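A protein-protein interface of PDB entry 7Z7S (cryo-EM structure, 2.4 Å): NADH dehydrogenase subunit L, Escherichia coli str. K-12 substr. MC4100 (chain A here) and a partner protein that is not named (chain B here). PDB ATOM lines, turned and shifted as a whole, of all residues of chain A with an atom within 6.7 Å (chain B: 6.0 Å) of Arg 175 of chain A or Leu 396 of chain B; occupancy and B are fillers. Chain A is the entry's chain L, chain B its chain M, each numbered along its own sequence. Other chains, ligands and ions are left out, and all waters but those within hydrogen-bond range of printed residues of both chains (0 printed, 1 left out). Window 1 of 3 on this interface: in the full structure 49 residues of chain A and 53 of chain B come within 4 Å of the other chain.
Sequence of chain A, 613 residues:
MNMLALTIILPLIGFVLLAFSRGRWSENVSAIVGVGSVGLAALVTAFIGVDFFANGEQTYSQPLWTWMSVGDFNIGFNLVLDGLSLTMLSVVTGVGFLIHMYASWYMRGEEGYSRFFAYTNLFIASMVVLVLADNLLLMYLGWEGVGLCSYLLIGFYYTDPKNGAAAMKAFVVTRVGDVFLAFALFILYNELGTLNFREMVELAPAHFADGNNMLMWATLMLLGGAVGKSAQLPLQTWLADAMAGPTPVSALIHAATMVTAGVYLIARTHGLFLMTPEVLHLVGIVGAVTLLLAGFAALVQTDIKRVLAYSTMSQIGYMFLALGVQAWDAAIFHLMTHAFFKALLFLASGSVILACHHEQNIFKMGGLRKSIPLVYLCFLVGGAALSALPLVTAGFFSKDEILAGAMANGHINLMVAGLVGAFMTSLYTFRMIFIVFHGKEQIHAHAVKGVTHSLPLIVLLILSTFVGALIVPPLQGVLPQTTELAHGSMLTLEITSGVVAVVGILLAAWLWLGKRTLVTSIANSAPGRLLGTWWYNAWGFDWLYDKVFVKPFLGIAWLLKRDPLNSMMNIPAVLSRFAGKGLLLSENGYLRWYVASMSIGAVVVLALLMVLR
The guanidinium group (NH1) of Arg 175 of chain A sits at hydrogen-bond distance from the backbone carbonyl oxygen (O) of Leu 396 of chain B, 3.1 Å away. The guanidinium group (NH2) of Arg 175 of chain A sits at hydrogen-bond distance from the backbone carbonyl oxygen (O) of Gly 397 of chain B (3.3 Å).
O of Val 430 of chain B is in hydrogen-bond range of OG of Ser 433 of chain B, at 3.1 Å. O of Asp 178 of chain A sits at hydrogen-bond distance from OH of Tyr 140 of chain A. The guanidinium group (NE) of Arg 175 of chain A is in salt-bridge range of the side-chain carboxylate (OE1) of Glu 144 of chain A. O of Phe 171 of chain A sits at hydrogen-bond distance from OG1 of Thr 174 of chain A (3.1 Å). The guanidinium group (NE) of Arg 175 of chain A lies within salt-bridge range of the side-chain carboxylate (OD1) of Asp 178 of chain A.
O of Glu 144 of chain A touches CE of Met 398 of chain B, 3.3 Å away. Glu 144 of chain A touches Pro 399 of chain B. Leu 148 of chain A touches Val 393 of chain B. Leu 148 of chain A touches Met 398 of chain B. Leu 396 of chain B touches Phe 171 of chain A. CE2 of Phe 171 of chain A touches CB of Ser 433 of chain B (3.8 Å). NH1 of Arg 175 of chain A touches O of Leu 429 of chain B, 3.7 Å away. Val 430 of chain B touches Arg 175 of chain A. Arg 175 of chain A touches Ser 433 of chain B (NH1 to CB, 3.4 Å). CG2 of Val 179 of chain A touches CG2 of Val 430 of chain B, 3.5 Å away.
Hydrophobic or aromatic side chains of chain B within 4 Å of the printed part of chain A: Val 393, Leu 396, Met 398, Pro 399, Phe 408, Leu 429, Val 430 and Leu 437. Among the printed residues, 16 pairs touch across the chains. Among the printed residues, no Asp or Glu carboxylate lies within 4 Å of a Lys or Arg side-chain nitrogen of the other chain.
Of the printed residues of chain B, Tyr 140 of chain A touches Phe 408. Of the printed residues of chain B, Glu 144 of chain A touches Met 398 and Pro 399. Of the printed residues of chain B, Val 176 of chain A touches Val 430 (3.8 Å). Leu 396 of chain B touches two residues of chain A. Printed residues of chain A within 4 Å of Ser 433 of chain B: Phe 171 (3.8 Å) and Arg 175 (3.4 Å). The nearest printed residue of chain A that does not touch Val 430 of chain B is Val 172 of chain A (4.9 Å).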
ATOM      1  N   TYR A 140     -23.575 -14.065 -19.836  1.00  0.00           N
ATOM      2  CA  TYR A 140     -22.598 -13.889 -18.767  1.00  0.00           C
ATOM      3  C   TYR A 140     -21.663 -15.085 -18.669  1.00  0.00           C
ATOM      4  O   TYR A 140     -20.478 -14.926 -18.365  1.00  0.00           O
ATOM      5  CB  TYR A 140     -23.322 -13.660 -17.443  1.00  0.00           C
ATOM      6  CG  TYR A 140     -22.482 -13.034 -16.365  1.00  0.00           C
ATOM      7  CD1 TYR A 140     -21.709 -13.816 -15.522  1.00  0.00           C
ATOM      8  CD2 TYR A 140     -22.469 -11.662 -16.179  1.00  0.00           C
ATOM      9  CE1 TYR A 140     -20.942 -13.250 -14.538  1.00  0.00           C
ATOM     10  CE2 TYR A 140     -21.705 -11.088 -15.195  1.00  0.00           C
ATOM     11  CZ  TYR A 140     -20.944 -11.887 -14.377  1.00  0.00           C
ATOM     12  OH  TYR A 140     -20.181 -11.324 -13.389  1.00  0.00           O
ATOM     13  N   GLU A 144     -17.650 -14.626 -19.004  1.00  0.00           N
ATOM     14  CA  GLU A 144     -16.620 -15.109 -18.093  1.00  0.00           C
ATOM     15  C   GLU A 144     -15.696 -16.101 -18.772  1.00  0.00           C
ATOM     16  O   GLU A 144     -14.499 -16.128 -18.476  1.00  0.00           O
ATOM     17  CB  GLU A 144     -17.253 -15.749 -16.864  1.00  0.00           C
ATOM     18  CG  GLU A 144     -18.206 -14.869 -16.114  1.00  0.00           C
ATOM     19  CD  GLU A 144     -17.661 -13.499 -15.870  1.00  0.00           C
ATOM     20  OE1 GLU A 144     -16.856 -13.354 -14.931  1.00  0.00           O
ATOM     21  OE2 GLU A 144     -18.045 -12.570 -16.607  1.00  0.00           O
ATOM     22  N   LEU A 148     -11.706 -15.680 -18.941  1.00  0.00           N
ATOM     23  CA  LEU A 148     -10.808 -16.709 -18.427  1.00  0.00           C
ATOM     24  C   LEU A 148      -9.854 -17.215 -19.503  1.00  0.00           C
ATOM     25  O   LEU A 148      -8.669 -17.439 -19.235  1.00  0.00           O
ATOM     26  CB  LEU A 148     -11.621 -17.866 -17.852  1.00  0.00           C
ATOM     27  CG  LEU A 148     -10.815 -19.057 -17.344  1.00  0.00           C
ATOM     28  CD1 LEU A 148      -9.993 -18.643 -16.145  1.00  0.00           C
ATOM     29  CD2 LEU A 148     -11.713 -20.232 -17.018  1.00  0.00           C
ATOM     30  N   LYS A 169      -3.531  -8.961 -14.254  1.00  0.00           N
ATOM     31  CA  LYS A 169      -4.115  -7.631 -14.373  1.00  0.00           C
ATOM     32  C   LYS A 169      -5.299  -7.628 -15.329  1.00  0.00           C
ATOM     33  O   LYS A 169      -6.329  -6.999 -15.050  1.00  0.00           O
ATOM     34  CB  LYS A 169      -3.053  -6.638 -14.833  1.00  0.00           C
ATOM     35  CG  LYS A 169      -3.521  -5.208 -14.890  1.00  0.00           C
ATOM     36  CD  LYS A 169      -2.962  -4.517 -16.110  1.00  0.00           C
ATOM     37  CE  LYS A 169      -1.959  -3.457 -15.720  1.00  0.00           C
ATOM     38  NZ  LYS A 169      -1.941  -2.349 -16.704  1.00  0.00           N
ATOM     39  N   ALA A 170      -5.174  -8.343 -16.452  1.00  0.00           N
ATOM     40  CA  ALA A 170      -6.276  -8.446 -17.405  1.00  0.00           C
ATOM     41  C   ALA A 170      -7.499  -9.088 -16.770  1.00  0.00           C
ATOM     42  O   ALA A 170      -8.618  -8.567 -16.881  1.00  0.00           O
ATOM     43  CB  ALA A 170      -5.837  -9.246 -18.625  1.00  0.00           C
ATOM     44  N   PHE A 171      -7.293 -10.206 -16.067  1.00  0.00           N
ATOM     45  CA  PHE A 171      -8.410 -10.901 -15.440  1.00  0.00           C
ATOM     46  C   PHE A 171      -9.059 -10.059 -14.350  1.00  0.00           C
ATOM     47  O   PHE A 171     -10.286 -10.043 -14.234  1.00  0.00           O
ATOM     48  CB  PHE A 171      -7.959 -12.246 -14.879  1.00  0.00           C
ATOM     49  CG  PHE A 171      -9.091 -13.194 -14.601  1.00  0.00           C
ATOM     50  CD1 PHE A 171      -9.741 -13.839 -15.635  1.00  0.00           C
ATOM     51  CD2 PHE A 171      -9.515 -13.428 -13.307  1.00  0.00           C
ATOM     52  CE1 PHE A 171     -10.779 -14.703 -15.381  1.00  0.00           C
ATOM     53  CE2 PHE A 171     -10.549 -14.294 -13.051  1.00  0.00           C
ATOM     54  CZ  PHE A 171     -11.182 -14.931 -14.088  1.00  0.00           C
ATOM     55  N   VAL A 172      -8.268  -9.323 -13.568  1.00  0.00           N
ATOM     56  CA  VAL A 172      -8.834  -8.548 -12.466  1.00  0.00           C
ATOM     57  C   VAL A 172      -9.644  -7.363 -12.991  1.00  0.00           C
ATOM     58  O   VAL A 172     -10.763  -7.108 -12.524  1.00  0.00           O
ATOM     59  CB  VAL A 172      -7.722  -8.107 -11.496  1.00  0.00           C
ATOM     60  CG1 VAL A 172      -8.188  -6.972 -10.603  1.00  0.00           C
ATOM     61  CG2 VAL A 172      -7.287  -9.278 -10.654  1.00  0.00           C
ATOM     62  N   VAL A 173      -9.105  -6.632 -13.974  1.00  0.00           N
ATOM     63  CA  VAL A 173      -9.833  -5.482 -14.513  1.00  0.00           C
ATOM     64  C   VAL A 173     -11.111  -5.930 -15.216  1.00  0.00           C
ATOM     65  O   VAL A 173     -12.195  -5.347 -15.018  1.00  0.00           O
ATOM     66  CB  VAL A 173      -8.926  -4.663 -15.448  1.00  0.00           C
ATOM     67  CG1 VAL A 173      -9.699  -3.526 -16.078  1.00  0.00           C
ATOM     68  CG2 VAL A 173      -7.749  -4.110 -14.684  1.00  0.00           C
ATOM     69  N   THR A 174     -11.025  -7.000 -16.008  1.00  0.00           N
ATOM     70  CA  THR A 174     -12.234  -7.491 -16.648  1.00  0.00           C
ATOM     71  C   THR A 174     -13.211  -8.070 -15.632  1.00  0.00           C
ATOM     72  O   THR A 174     -14.413  -7.992 -15.847  1.00  0.00           O
ATOM     73  CB  THR A 174     -11.887  -8.509 -17.727  1.00  0.00           C
ATOM     74  OG1 THR A 174     -11.030  -9.516 -17.185  1.00  0.00           O
ATOM     75  CG2 THR A 174     -11.173  -7.814 -18.864  1.00  0.00           C
ATOM     76  N   ARG A 175     -12.729  -8.593 -14.501  1.00  0.00           N
ATOM     77  CA  ARG A 175     -13.638  -9.088 -13.469  1.00  0.00           C
ATOM     78  C   ARG A 175     -14.375  -7.956 -12.761  1.00  0.00           C
ATOM     79  O   ARG A 175     -15.526  -8.136 -12.348  1.00  0.00           O
ATOM     80  CB  ARG A 175     -12.869  -9.934 -12.458  1.00  0.00           C
ATOM     81  CG  ARG A 175     -13.692 -11.027 -11.816  1.00  0.00           C
ATOM     82  CD  ARG A 175     -13.513 -12.346 -12.536  1.00  0.00           C
ATOM     83  NE  ARG A 175     -14.711 -13.172 -12.490  1.00  0.00           N
ATOM     84  CZ  ARG A 175     -15.059 -13.937 -11.465  1.00  0.00           C
ATOM     85  NH1 ARG A 175     -14.332 -13.990 -10.364  1.00  0.00           N
ATOM     86  NH2 ARG A 175     -16.162 -14.670 -11.549  1.00  0.00           N
ATOM     87  N   VAL A 176     -13.735  -6.797 -12.603  1.00  0.00           N
ATOM     88  CA  VAL A 176     -14.459  -5.611 -12.137  1.00  0.00           C
ATOM     89  C   VAL A 176     -15.559  -5.245 -13.131  1.00  0.00           C
ATOM     90  O   VAL A 176     -16.695  -4.906 -12.747  1.00  0.00           O
ATOM     91  CB  VAL A 176     -13.481  -4.444 -11.905  1.00  0.00           C
ATOM     92  CG1 VAL A 176     -14.223  -3.188 -11.487  1.00  0.00           C
ATOM     93  CG2 VAL A 176     -12.454  -4.814 -10.860  1.00  0.00           C
ATOM     94  N   GLY A 177     -15.246  -5.343 -14.427  1.00  0.00           N
ATOM     95  CA  GLY A 177     -16.283  -5.189 -15.443  1.00  0.00           C
ATOM     96  C   GLY A 177     -17.428  -6.182 -15.302  1.00  0.00           C
ATOM     97  O   GLY A 177     -18.600  -5.815 -15.421  1.00  0.00           O
ATOM     98  N   ASP A 178     -17.107  -7.449 -15.038  1.00  0.00           N
ATOM     99  CA  ASP A 178     -18.142  -8.465 -14.848  1.00  0.00           C
ATOM    100  C   ASP A 178     -18.965  -8.230 -13.591  1.00  0.00           C
ATOM    101  O   ASP A 178     -20.128  -8.627 -13.540  1.00  0.00           O
ATOM    102  CB  ASP A 178     -17.537  -9.866 -14.810  1.00  0.00           C
ATOM    103  CG  ASP A 178     -16.482 -10.075 -15.861  1.00  0.00           C
ATOM    104  OD1 ASP A 178     -15.610 -10.943 -15.672  1.00  0.00           O
ATOM    105  OD2 ASP A 178     -16.550  -9.403 -16.909  1.00  0.00           O
ATOM    106  N   VAL A 179     -18.390  -7.599 -12.570  1.00  0.00           N
ATOM    107  CA  VAL A 179     -19.182  -7.226 -11.401  1.00  0.00           C
ATOM    108  C   VAL A 179     -20.193  -6.141 -11.752  1.00  0.00           C
ATOM    109  O   VAL A 179     -21.352  -6.187 -11.310  1.00  0.00           O
ATOM    110  CB  VAL A 179     -18.258  -6.823 -10.242  1.00  0.00           C
ATOM    111  CG1 VAL A 179     -19.033  -6.235  -9.102  1.00  0.00           C
ATOM    112  CG2 VAL A 179     -17.600  -8.059  -9.731  1.00  0.00           C
ATOM    113  N   PHE A 180     -19.792  -5.165 -12.570  1.00  0.00           N
ATOM    114  CA  PHE A 180     -20.774  -4.181 -13.038  1.00  0.00           C
ATOM    115  C   PHE A 180     -21.869  -4.839 -13.878  1.00  0.00           C
ATOM    116  O   PHE A 180     -23.060  -4.526 -13.729  1.00  0.00           O
ATOM    117  CB  PHE A 180     -20.085  -3.075 -13.829  1.00  0.00           C
ATOM    118  CG  PHE A 180     -19.101  -2.291 -13.028  1.00  0.00           C
ATOM    119  CD1 PHE A 180     -19.329  -2.038 -11.690  1.00  0.00           C
ATOM    120  CD2 PHE A 180     -17.938  -1.821 -13.606  1.00  0.00           C
ATOM    121  CE1 PHE A 180     -18.420  -1.329 -10.947  1.00  0.00           C
ATOM    122  CE2 PHE A 180     -17.026  -1.108 -12.867  1.00  0.00           C
ATOM    123  CZ  PHE A 180     -17.270  -0.862 -11.533  1.00  0.00           C
ATOM    124  N   GLY A 228     -15.551  -2.638 -19.412  1.00  0.00           N
ATOM    125  CA  GLY A 228     -14.600  -3.584 -18.864  1.00  0.00           C
ATOM    126  C   GLY A 228     -14.119  -4.585 -19.895  1.00  0.00           C
ATOM    127  O   GLY A 228     -12.921  -4.858 -19.994  1.00  0.00           O
ATOM    128  N   LYS A 229     -15.041  -5.140 -20.680  1.00  0.00           N
ATOM    129  CA  LYS A 229     -14.629  -6.146 -21.654  1.00  0.00           C
ATOM    130  C   LYS A 229     -13.964  -5.526 -22.879  1.00  0.00           C
ATOM    131  O   LYS A 229     -13.038  -6.113 -23.447  1.00  0.00           O
ATOM    132  CB  LYS A 229     -15.828  -6.988 -22.074  1.00  0.00           C
ATOM    133  CG  LYS A 229     -15.463  -8.291 -22.733  1.00  0.00           C
ATOM    134  CD  LYS A 229     -14.599  -9.137 -21.830  1.00  0.00           C
ATOM    135  CE  LYS A 229     -15.413  -9.821 -20.761  1.00  0.00           C
ATOM    136  NZ  LYS A 229     -14.564 -10.525 -19.773  1.00  0.00           N
ATOM    137  N   HIS B 322     -16.298 -18.095   1.279  1.00  0.00           N
ATOM    138  CA  HIS B 322     -17.483 -18.698   0.672  1.00  0.00           C
ATOM    139  C   HIS B 322     -18.596 -18.884   1.696  1.00  0.00           C
ATOM    140  O   HIS B 322     -19.786 -18.701   1.388  1.00  0.00           O
ATOM    141  CB  HIS B 322     -17.114 -20.027   0.023  1.00  0.00           C
ATOM    142  CG  HIS B 322     -16.027 -19.913  -0.998  1.00  0.00           C
ATOM    143  ND1 HIS B 322     -15.178 -20.955  -1.299  1.00  0.00           N
ATOM    144  CD2 HIS B 322     -15.648 -18.880  -1.785  1.00  0.00           C
ATOM    145  CE1 HIS B 322     -14.322 -20.567  -2.228  1.00  0.00           C
ATOM    146  NE2 HIS B 322     -14.587 -19.311  -2.538  1.00  0.00           N
ATOM    147  N   PHE B 391      -9.612 -26.236 -10.278  1.00  0.00           N
ATOM    148  CA  PHE B 391     -10.306 -26.043  -9.009  1.00  0.00           C
ATOM    149  C   PHE B 391     -10.163 -24.621  -8.482  1.00  0.00           C
ATOM    150  O   PHE B 391     -11.094 -24.104  -7.859  1.00  0.00           O
ATOM    151  CB  PHE B 391      -9.825 -27.066  -7.984  1.00  0.00           C
ATOM    152  CG  PHE B 391     -10.530 -28.379  -8.092  1.00  0.00           C
ATOM    153  CD1 PHE B 391     -11.848 -28.502  -7.704  1.00  0.00           C
ATOM    154  CD2 PHE B 391      -9.889 -29.481  -8.618  1.00  0.00           C
ATOM    155  CE1 PHE B 391     -12.504 -29.705  -7.820  1.00  0.00           C
ATOM    156  CE2 PHE B 391     -10.542 -30.685  -8.735  1.00  0.00           C
ATOM    157  CZ  PHE B 391     -11.849 -30.796  -8.335  1.00  0.00           C
ATOM    158  N   ALA B 392      -9.031 -23.963  -8.739  1.00  0.00           N
ATOM    159  CA  ALA B 392      -8.919 -22.546  -8.415  1.00  0.00           C
ATOM    160  C   ALA B 392      -9.813 -21.700  -9.307  1.00  0.00           C
ATOM    161  O   ALA B 392     -10.301 -20.651  -8.879  1.00  0.00           O
ATOM    162  CB  ALA B 392      -7.466 -22.094  -8.535  1.00  0.00           C
ATOM    163  N   VAL B 393     -10.024 -22.136 -10.547  1.00  0.00           N
ATOM    164  CA  VAL B 393     -10.990 -21.501 -11.430  1.00  0.00           C
ATOM    165  C   VAL B 393     -12.403 -21.662 -10.883  1.00  0.00           C
ATOM    166  O   VAL B 393     -13.206 -20.725 -10.912  1.00  0.00           O
ATOM    167  CB  VAL B 393     -10.823 -22.080 -12.848  1.00  0.00           C
ATOM    168  CG1 VAL B 393     -12.100 -22.049 -13.624  1.00  0.00           C
ATOM    169  CG2 VAL B 393      -9.756 -21.307 -13.595  1.00  0.00           C
ATOM    170  N   ALA B 394     -12.717 -22.843 -10.352  1.00  0.00           N
ATOM    171  CA  ALA B 394     -14.024 -23.065  -9.744  1.00  0.00           C
ATOM    172  C   ALA B 394     -14.224 -22.198  -8.504  1.00  0.00           C
ATOM    173  O   ALA B 394     -15.300 -21.626  -8.312  1.00  0.00           O
ATOM    174  CB  ALA B 394     -14.202 -24.541  -9.400  1.00  0.00           C
ATOM    175  N   THR B 395     -13.195 -22.061  -7.665  1.00  0.00           N
ATOM    176  CA  THR B 395     -13.369 -21.343  -6.406  1.00  0.00           C
ATOM    177  C   THR B 395     -13.510 -19.835  -6.570  1.00  0.00           C
ATOM    178  O   THR B 395     -13.863 -19.164  -5.596  1.00  0.00           O
ATOM    179  CB  THR B 395     -12.212 -21.625  -5.448  1.00  0.00           C
ATOM    180  OG1 THR B 395     -10.967 -21.343  -6.090  1.00  0.00           O
ATOM    181  CG2 THR B 395     -12.232 -23.070  -5.009  1.00  0.00           C
ATOM    182  N   LEU B 396     -13.246 -19.277  -7.745  1.00  0.00           N
ATOM    183  CA  LEU B 396     -13.536 -17.869  -7.959  1.00  0.00           C
ATOM    184  C   LEU B 396     -14.922 -17.640  -8.545  1.00  0.00           C
ATOM    185  O   LEU B 396     -15.285 -16.492  -8.813  1.00  0.00           O
ATOM    186  CB  LEU B 396     -12.466 -17.219  -8.848  1.00  0.00           C
ATOM    187  CG  LEU B 396     -12.126 -17.742 -10.242  1.00  0.00           C
ATOM    188  CD1 LEU B 396     -12.923 -17.029 -11.321  1.00  0.00           C
ATOM    189  CD2 LEU B 396     -10.643 -17.587 -10.497  1.00  0.00           C
ATOM    190  N   GLY B 397     -15.709 -18.694  -8.730  1.00  0.00           N
ATOM    191  CA  GLY B 397     -17.060 -18.538  -9.224  1.00  0.00           C
ATOM    192  C   GLY B 397     -17.131 -18.503 -10.732  1.00  0.00           C
ATOM    193  O   GLY B 397     -17.717 -17.593 -11.319  1.00  0.00           O
ATOM    194  N   MET B 398     -16.544 -19.465 -11.350  1.00  0.00           N
ATOM    195  CA  MET B 398     -16.542 -19.606 -12.797  1.00  0.00           C
ATOM    196  C   MET B 398     -17.835 -20.249 -13.272  1.00  0.00           C
ATOM    197  O   MET B 398     -18.199 -21.322 -12.779  1.00  0.00           O
ATOM    198  CB  MET B 398     -15.376 -20.456 -13.244  1.00  0.00           C
ATOM    199  CG  MET B 398     -15.102 -20.385 -14.704  1.00  0.00           C
ATOM    200  SD  MET B 398     -14.795 -18.726 -15.279  1.00  0.00           S
ATOM    201  CE  MET B 398     -15.331 -18.984 -16.949  1.00  0.00           C
ATOM    202  N   PRO B 399     -18.556 -19.615 -14.196  1.00  0.00           N
ATOM    203  CA  PRO B 399     -19.677 -20.291 -14.853  1.00  0.00           C
ATOM    204  C   PRO B 399     -19.215 -21.548 -15.569  1.00  0.00           C
ATOM    205  O   PRO B 399     -18.149 -21.581 -16.184  1.00  0.00           O
ATOM    206  CB  PRO B 399     -20.193 -19.238 -15.833  1.00  0.00           C
ATOM    207  CG  PRO B 399     -19.816 -17.967 -15.238  1.00  0.00           C
ATOM    208  CD  PRO B 399     -18.524 -18.181 -14.514  1.00  0.00           C
ATOM    209  N   ASN B 403     -20.075 -23.486  -8.298  1.00  0.00           N
ATOM    210  CA  ASN B 403     -19.797 -22.341  -7.441  1.00  0.00           C
ATOM    211  C   ASN B 403     -20.442 -21.078  -7.987  1.00  0.00           C
ATOM    212  O   ASN B 403     -20.974 -20.265  -7.224  1.00  0.00           O
ATOM    213  CB  ASN B 403     -18.291 -22.139  -7.307  1.00  0.00           C
ATOM    214  CG  ASN B 403     -17.589 -23.321  -6.677  1.00  0.00           C
ATOM    215  OD1 ASN B 403     -17.306 -23.319  -5.484  1.00  0.00           O
ATOM    216  ND2 ASN B 403     -17.288 -24.330  -7.479  1.00  0.00           N
ATOM    217  N   GLU B 407     -23.273 -18.960  -5.978  1.00  0.00           N
ATOM    218  CA  GLU B 407     -22.951 -17.578  -5.640  1.00  0.00           C
ATOM    219  C   GLU B 407     -23.893 -16.597  -6.323  1.00  0.00           C
ATOM    220  O   GLU B 407     -24.400 -15.666  -5.688  1.00  0.00           O
ATOM    221  CB  GLU B 407     -21.501 -17.277  -6.020  1.00  0.00           C
ATOM    222  CG  GLU B 407     -20.550 -17.230  -4.836  1.00  0.00           C
ATOM    223  CD  GLU B 407     -19.120 -17.605  -5.203  1.00  0.00           C
ATOM    224  OE1 GLU B 407     -18.900 -18.130  -6.314  1.00  0.00           O
ATOM    225  OE2 GLU B 407     -18.216 -17.377  -4.373  1.00  0.00           O
ATOM    226  N   PHE B 408     -24.193 -16.821  -7.599  1.00  0.00           N
ATOM    227  CA  PHE B 408     -25.017 -15.870  -8.317  1.00  0.00           C
ATOM    228  C   PHE B 408     -26.489 -15.982  -7.963  1.00  0.00           C
ATOM    229  O   PHE B 408     -27.177 -14.961  -7.947  1.00  0.00           O
ATOM    230  CB  PHE B 408     -24.802 -16.019  -9.816  1.00  0.00           C
ATOM    231  CG  PHE B 408     -23.905 -14.971 -10.375  1.00  0.00           C
ATOM    232  CD1 PHE B 408     -22.605 -14.851  -9.915  1.00  0.00           C
ATOM    233  CD2 PHE B 408     -24.363 -14.079 -11.324  1.00  0.00           C
ATOM    234  CE1 PHE B 408     -21.771 -13.881 -10.410  1.00  0.00           C
ATOM    235  CE2 PHE B 408     -23.533 -13.104 -11.821  1.00  0.00           C
ATOM    236  CZ  PHE B 408     -22.234 -13.005 -11.358  1.00  0.00           C
ATOM    237  N   LEU B 429     -16.503 -11.054  -4.753  1.00  0.00           N
ATOM    238  CA  LEU B 429     -16.211 -12.034  -5.806  1.00  0.00           C
ATOM    239  C   LEU B 429     -14.981 -11.625  -6.627  1.00  0.00           C
ATOM    240  O   LEU B 429     -14.176 -12.481  -7.038  1.00  0.00           O
ATOM    241  CB  LEU B 429     -17.449 -12.217  -6.686  1.00  0.00           C
ATOM    242  CG  LEU B 429     -17.467 -12.882  -8.057  1.00  0.00           C
ATOM    243  CD1 LEU B 429     -18.813 -13.543  -8.220  1.00  0.00           C
ATOM    244  CD2 LEU B 429     -17.255 -11.880  -9.171  1.00  0.00           C
ATOM    245  N   VAL B 430     -14.821 -10.318  -6.869  1.00  0.00           N
ATOM    246  CA  VAL B 430     -13.548  -9.824  -7.430  1.00  0.00           C
ATOM    247  C   VAL B 430     -12.363 -10.206  -6.538  1.00  0.00           C
ATOM    248  O   VAL B 430     -11.312 -10.664  -7.024  1.00  0.00           O
ATOM    249  CB  VAL B 430     -13.601  -8.301  -7.671  1.00  0.00           C
ATOM    250  CG1 VAL B 430     -12.216  -7.681  -7.635  1.00  0.00           C
ATOM    251  CG2 VAL B 430     -14.133  -8.036  -9.025  1.00  0.00           C
ATOM    252  N   ALA B 432     -12.159 -12.727  -4.589  1.00  0.00           N
ATOM    253  CA  ALA B 432     -11.961 -14.166  -4.747  1.00  0.00           C
ATOM    254  C   ALA B 432     -11.117 -14.489  -5.973  1.00  0.00           C
ATOM    255  O   ALA B 432     -10.214 -15.340  -5.913  1.00  0.00           O
ATOM    256  CB  ALA B 432     -13.307 -14.876  -4.834  1.00  0.00           C
ATOM    257  N   SER B 433     -11.405 -13.821  -7.093  1.00  0.00           N
ATOM    258  CA  SER B 433     -10.581 -14.003  -8.288  1.00  0.00           C
ATOM    259  C   SER B 433      -9.133 -13.599  -8.027  1.00  0.00           C
ATOM    260  O   SER B 433      -8.198 -14.256  -8.513  1.00  0.00           O
ATOM    261  CB  SER B 433     -11.160 -13.207  -9.455  1.00  0.00           C
ATOM    262  OG  SER B 433     -10.465 -11.991  -9.640  1.00  0.00           O
ATOM    263  N   TYR B 435      -7.427 -13.764  -5.084  1.00  0.00           N
ATOM    264  CA  TYR B 435      -6.652 -14.741  -4.310  1.00  0.00           C
ATOM    265  C   TYR B 435      -6.447 -16.046  -5.078  1.00  0.00           C
ATOM    266  O   TYR B 435      -5.412 -16.703  -4.904  1.00  0.00           O
ATOM    267  CB  TYR B 435      -7.251 -15.000  -2.907  1.00  0.00           C
ATOM    268  CG  TYR B 435      -8.649 -15.599  -2.736  1.00  0.00           C
ATOM    269  CD1 TYR B 435      -9.013 -16.814  -3.300  1.00  0.00           C
ATOM    270  CD2 TYR B 435      -9.583 -14.962  -1.947  1.00  0.00           C
ATOM    271  CE1 TYR B 435     -10.266 -17.329  -3.142  1.00  0.00           C
ATOM    272  CE2 TYR B 435     -10.836 -15.492  -1.750  1.00  0.00           C
ATOM    273  CZ  TYR B 435     -11.171 -16.677  -2.357  1.00  0.00           C
ATOM    274  OH  TYR B 435     -12.420 -17.214  -2.185  1.00  0.00           O
ATOM    275  N   SER B 436      -7.394 -16.422  -5.948  1.00  0.00           N
ATOM    276  CA  SER B 436      -7.216 -17.644  -6.729  1.00  0.00           C
ATOM    277  C   SER B 436      -6.077 -17.502  -7.731  1.00  0.00           C
ATOM    278  O   SER B 436      -5.239 -18.407  -7.862  1.00  0.00           O
ATOM    279  CB  SER B 436      -8.515 -18.010  -7.438  1.00  0.00           C
ATOM    280  OG  SER B 436      -9.476 -18.480  -6.516  1.00  0.00           O
ATOM    281  N   LEU B 437      -6.020 -16.364  -8.432  1.00  0.00           N
ATOM    282  CA  LEU B 437      -4.907 -16.121  -9.343  1.00  0.00           C
ATOM    283  C   LEU B 437      -3.583 -16.031  -8.602  1.00  0.00           C
ATOM    284  O   LEU B 437      -2.557 -16.500  -9.107  1.00  0.00           O
ATOM    285  CB  LEU B 437      -5.137 -14.850 -10.154  1.00  0.00           C
ATOM    286  CG  LEU B 437      -5.966 -14.818 -11.437  1.00  0.00           C
ATOM    287  CD1 LEU B 437      -7.154 -15.761 -11.446  1.00  0.00           C
ATOM    288  CD2 LEU B 437      -6.406 -13.381 -11.649  1.00  0.00           C
